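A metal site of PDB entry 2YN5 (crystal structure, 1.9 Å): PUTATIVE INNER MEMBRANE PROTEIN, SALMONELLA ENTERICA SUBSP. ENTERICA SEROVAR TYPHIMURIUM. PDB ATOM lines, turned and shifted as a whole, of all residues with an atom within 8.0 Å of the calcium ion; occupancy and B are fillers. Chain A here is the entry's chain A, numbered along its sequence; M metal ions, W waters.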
ATOM      1  N   LEU A  90      -1.132 -14.386  23.237  1.00  0.00           N
ATOM      2  CA  LEU A  90      -1.854 -14.593  21.977  1.00  0.00           C
ATOM      3  C   LEU A  90      -1.528 -13.419  21.047  1.00  0.00           C
ATOM      4  O   LEU A  90      -1.699 -12.246  21.445  1.00  0.00           O
ATOM      5  CB  LEU A  90      -3.353 -14.659  22.253  1.00  0.00           C
ATOM      6  CG  LEU A  90      -4.271 -14.940  21.056  1.00  0.00           C
ATOM      7  CD1 LEU A  90      -3.977 -16.335  20.490  1.00  0.00           C
ATOM      8  CD2 LEU A  90      -5.745 -14.782  21.429  1.00  0.00           C
ATOM      9  N   PRO A  92      -1.845 -10.495  18.505  1.00  0.00           N
ATOM     10  CA  PRO A  92      -3.032  -9.698  18.172  1.00  0.00           C
ATOM     11  C   PRO A  92      -3.646 -10.168  16.859  1.00  0.00           C
ATOM     12  O   PRO A  92      -4.869 -10.266  16.740  1.00  0.00           O
ATOM     13  CB  PRO A  92      -2.494  -8.256  18.057  1.00  0.00           C
ATOM     14  CG  PRO A  92      -1.240  -8.264  18.861  1.00  0.00           C
ATOM     15  CD  PRO A  92      -0.658  -9.652  18.738  1.00  0.00           C
ATOM     16  N   SER A  94      -4.003 -13.046  15.805  1.00  0.00           N
ATOM     17  CA  SER A  94      -4.778 -14.276  15.988  1.00  0.00           C
ATOM     18  C   SER A  94      -5.895 -14.124  17.015  1.00  0.00           C
ATOM     19  O   SER A  94      -6.427 -15.131  17.482  1.00  0.00           O
ATOM     20  CB  SER A  94      -3.863 -15.415  16.451  1.00  0.00           C
ATOM     21  OG  SER A  94      -2.915 -15.771  15.473  1.00  0.00           O
ATOM     22  N   ASP A  95      -6.242 -12.882  17.367  1.00  0.00           N
ATOM     23  CA  ASP A  95      -7.233 -12.615  18.407  1.00  0.00           C
ATOM     24  C   ASP A  95      -8.502 -12.044  17.781  1.00  0.00           C
ATOM     25  O   ASP A  95      -8.655 -10.833  17.681  1.00  0.00           O
ATOM     26  CB  ASP A  95      -6.671 -11.627  19.433  1.00  0.00           C
ATOM     27  CG  ASP A  95      -7.653 -11.293  20.532  1.00  0.00           C
ATOM     28  OD1 ASP A  95      -8.759 -11.886  20.577  1.00  0.00           O
ATOM     29  OD2 ASP A  95      -7.303 -10.438  21.369  1.00  0.00           O
ATOM     30  N   SER A  96      -9.414 -12.937  17.376  1.00  0.00           N
ATOM     31  CA  SER A  96     -10.582 -12.552  16.604  1.00  0.00           C
ATOM     32  C   SER A  96     -11.645 -11.886  17.493  1.00  0.00           C
ATOM     33  O   SER A  96     -11.573 -11.968  18.720  1.00  0.00           O
ATOM     34  CB  SER A  96     -11.152 -13.787  15.885  1.00  0.00           C
ATOM     35  OG  SER A  96     -11.915 -14.561  16.818  1.00  0.00           O
ATOM     36  N   GLY A  97     -12.645 -11.277  16.874  1.00  0.00           N
ATOM     37  CA  GLY A  97     -13.723 -10.628  17.626  1.00  0.00           C
ATOM     38  C   GLY A  97     -13.254  -9.599  18.647  1.00  0.00           C
ATOM     39  O   GLY A  97     -12.312  -8.853  18.391  1.00  0.00           O
ATOM     40  N   THR A  98     -13.900  -9.571  19.804  1.00  0.00           N
ATOM     41  CA  THR A  98     -13.503  -8.663  20.880  1.00  0.00           C
ATOM     42  C   THR A  98     -11.978  -8.791  21.071  1.00  0.00           C
ATOM     43  O   THR A  98     -11.460  -9.903  21.148  1.00  0.00           O
ATOM     44  CB  THR A  98     -14.240  -8.989  22.198  1.00  0.00           C
ATOM     45  OG1 THR A  98     -15.654  -9.200  21.934  1.00  0.00           O
ATOM     46  CG2 THR A  98     -14.065  -7.868  23.186  1.00  0.00           C
ATOM     47  N   VAL A  99     -11.261  -7.671  21.100  1.00  0.00           N
ATOM     48  CA  VAL A  99      -9.803  -7.738  21.165  1.00  0.00           C
ATOM     49  C   VAL A  99      -9.312  -7.806  22.623  1.00  0.00           C
ATOM     50  O   VAL A  99      -9.817  -7.099  23.495  1.00  0.00           O
ATOM     51  CB  VAL A  99      -9.139  -6.590  20.376  1.00  0.00           C
ATOM     52  CG1 VAL A  99      -7.612  -6.705  20.394  1.00  0.00           C
ATOM     53  CG2 VAL A  99      -9.628  -6.575  18.924  1.00  0.00           C
ATOM     54  N   GLY A 100      -8.354  -8.706  22.888  1.00  0.00           N
ATOM     55  CA  GLY A 100      -7.689  -8.790  24.189  1.00  0.00           C
ATOM     56  C   GLY A 100      -8.333  -9.642  25.271  1.00  0.00           C
ATOM     57  O   GLY A 100      -7.971  -9.506  26.447  1.00  0.00           O
ATOM     58  N   ASP A 101      -9.265 -10.516  24.872  1.00  0.00           N
ATOM     59  CA  ASP A 101      -9.964 -11.405  25.813  1.00  0.00           C
ATOM     60  C   ASP A 101      -9.506 -12.862  25.782  1.00  0.00           C
ATOM     61  O   ASP A 101     -10.149 -13.710  26.379  1.00  0.00           O
ATOM     62  CB  ASP A 101     -11.486 -11.363  25.600  1.00  0.00           C
ATOM     63  CG  ASP A 101     -11.904 -11.824  24.196  1.00  0.00           C
ATOM     64  OD1 ASP A 101     -11.040 -12.202  23.372  1.00  0.00           O
ATOM     65  OD2 ASP A 101     -13.128 -11.789  23.925  1.00  0.00           O
ATOM     66  N   ASN A 102      -8.422 -13.126  25.059  1.00  0.00           N
ATOM     67  CA  ASN A 102      -7.895 -14.477  24.866  1.00  0.00           C
ATOM     68  C   ASN A 102      -8.917 -15.484  24.333  1.00  0.00           C
ATOM     69  O   ASN A 102      -8.848 -16.660  24.643  1.00  0.00           O
ATOM     70  CB  ASN A 102      -7.233 -14.964  26.164  1.00  0.00           C
ATOM     71  CG  ASN A 102      -5.815 -14.446  26.322  1.00  0.00           C
ATOM     72  OD1 ASN A 102      -5.212 -13.932  25.381  1.00  0.00           O
ATOM     73  ND2 ASN A 102      -5.272 -14.577  27.513  1.00  0.00           N
ATOM     74  N   ILE A 103      -9.908 -15.002  23.567  1.00  0.00           N
ATOM     75  CA  ILE A 103     -10.899 -15.874  22.954  1.00  0.00           C
ATOM     76  C   ILE A 103     -10.748 -15.639  21.445  1.00  0.00           C
ATOM     77  O   ILE A 103     -10.700 -14.498  21.006  1.00  0.00           O
ATOM     78  CB  ILE A 103     -12.328 -15.502  23.423  1.00  0.00           C
ATOM     79  CG1 ILE A 103     -12.479 -15.737  24.931  1.00  0.00           C
ATOM     80  CG2 ILE A 103     -13.385 -16.333  22.689  1.00  0.00           C
ATOM     81  CD1 ILE A 103     -13.705 -15.047  25.514  1.00  0.00           C
ATOM     82  N   THR A 104     -10.635 -16.715  20.672  1.00  0.00           N
ATOM     83  CA  THR A 104     -10.469 -16.552  19.206  1.00  0.00           C
ATOM     84  C   THR A 104     -11.106 -17.687  18.414  1.00  0.00           C
ATOM     85  O   THR A 104     -11.211 -18.845  18.872  1.00  0.00           O
ATOM     86  CB  THR A 104      -8.990 -16.353  18.812  1.00  0.00           C
ATOM     87  OG1 THR A 104      -8.877 -16.069  17.390  1.00  0.00           O
ATOM     88  CG2 THR A 104      -8.155 -17.598  19.158  1.00  0.00           C
ATOM     89  N   ARG A 105     -11.568 -17.334  17.215  1.00  0.00           N
ATOM     90  CA  ARG A 105     -12.017 -18.323  16.244  1.00  0.00           C
ATOM     91  C   ARG A 105     -10.872 -18.955  15.432  1.00  0.00           C
ATOM     92  O   ARG A 105     -11.088 -19.985  14.760  1.00  0.00           O
ATOM     93  CB  ARG A 105     -13.033 -17.651  15.301  1.00  0.00           C
ATOM     94  CG  ARG A 105     -12.389 -16.701  14.317  1.00  0.00           C
ATOM     95  CD  ARG A 105     -13.395 -15.819  13.563  1.00  0.00           C
ATOM     96  NE  ARG A 105     -14.372 -16.643  12.848  1.00  0.00           N
ATOM     97  CZ  ARG A 105     -14.224 -17.073  11.590  1.00  0.00           C
ATOM     98  NH1 ARG A 105     -13.142 -16.765  10.892  1.00  0.00           N
ATOM     99  NH2 ARG A 105     -15.168 -17.815  11.040  1.00  0.00           N
ATOM    100  N   THR A 177      -9.311 -19.467  24.761  1.00  0.00           N
ATOM    101  CA  THR A 177     -10.509 -20.206  24.369  1.00  0.00           C
ATOM    102  C   THR A 177     -10.630 -20.185  22.859  1.00  0.00           C
ATOM    103  O   THR A 177     -10.656 -19.111  22.272  1.00  0.00           O
ATOM    104  CB  THR A 177     -11.794 -19.560  24.954  1.00  0.00           C
ATOM    105  OG1 THR A 177     -11.744 -19.653  26.376  1.00  0.00           O
ATOM    106  CG2 THR A 177     -13.035 -20.300  24.481  1.00  0.00           C
ATOM    107  N   ARG A 267     -18.990 -13.419  20.409  1.00  0.00           N
ATOM    108  CA  ARG A 267     -17.840 -12.639  20.917  1.00  0.00           C
ATOM    109  C   ARG A 267     -16.521 -12.993  20.210  1.00  0.00           C
ATOM    110  O   ARG A 267     -15.614 -12.170  20.173  1.00  0.00           O
ATOM    111  CB  ARG A 267     -17.691 -12.872  22.412  1.00  0.00           C
ATOM    112  CG  ARG A 267     -17.570 -14.344  22.714  1.00  0.00           C
ATOM    113  CD  ARG A 267     -17.430 -14.616  24.199  1.00  0.00           C
ATOM    114  NE  ARG A 267     -17.206 -16.049  24.362  1.00  0.00           N
ATOM    115  CZ  ARG A 267     -17.055 -16.654  25.541  1.00  0.00           C
ATOM    116  NH1 ARG A 267     -17.098 -15.970  26.674  1.00  0.00           N
ATOM    117  NH2 ARG A 267     -16.842 -17.966  25.560  1.00  0.00           N
ATOM    118  N   ALA A 268     -16.424 -14.204  19.672  1.00  0.00           N
ATOM    119  CA  ALA A 268     -15.244 -14.643  18.919  1.00  0.00           C
ATOM    120  C   ALA A 268     -15.232 -14.125  17.460  1.00  0.00           C
ATOM    121  O   ALA A 268     -14.253 -14.313  16.710  1.00  0.00           O
ATOM    122  CB  ALA A 268     -15.142 -16.166  18.940  1.00  0.00           C
ATOM    123  N   GLY A 269     -16.307 -13.461  17.056  1.00  0.00           N
ATOM    124  CA  GLY A 269     -16.391 -12.948  15.683  1.00  0.00           C
ATOM    125  C   GLY A 269     -16.933 -13.935  14.656  1.00  0.00           C
ATOM    126  O   GLY A 269     -16.943 -13.640  13.450  1.00  0.00           O
HETATM  127 CA    CA M   1     -10.995 -12.215  20.945  1.00  0.00          CA
HETATM  128  O   HOH W   1     -13.211 -12.632  21.454  1.00  0.00           O
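N of Gly 100 is in hydrogen-bond range of OD2 of Asp 95, at 2.5 Å.
The backbone NH (N) of Ser 96 sits at hydrogen-bond distance from the side-chain hydroxyl (OG1) of Thr 104, at 3.2 Å.
N of Arg 105 lies within hydrogen-bond range of OG of Ser 96.
N of Thr 98 sits at hydrogen-bond distance from O of Arg 267, 3.1 Å away.
Of the 18 residues printed, 5 come within 4 Å of the calcium ion.
The nearest printed residue that does not touch the calcium ion is Gly 97 (4.2 Å).
The calcium ion is bound by the side-chain carboxylate of Asp 95 (2.3 Å), the backbone carbonyl oxygen of Ile 103 (2.3 Å), the backbone carbonyl oxygen of Ser 96 (2.3 Å), water W1 (2.3 Å), the backbone carbonyl oxygen of Thr 98 (2.4 Å) and the side-chain carboxylate of Asp 101 (2.4 Å).
The calcium ion has six donor atoms within binding distance.
Water W1 lies within hydrogen-bond range of OD2 of Asp 101 and O of Arg 267.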
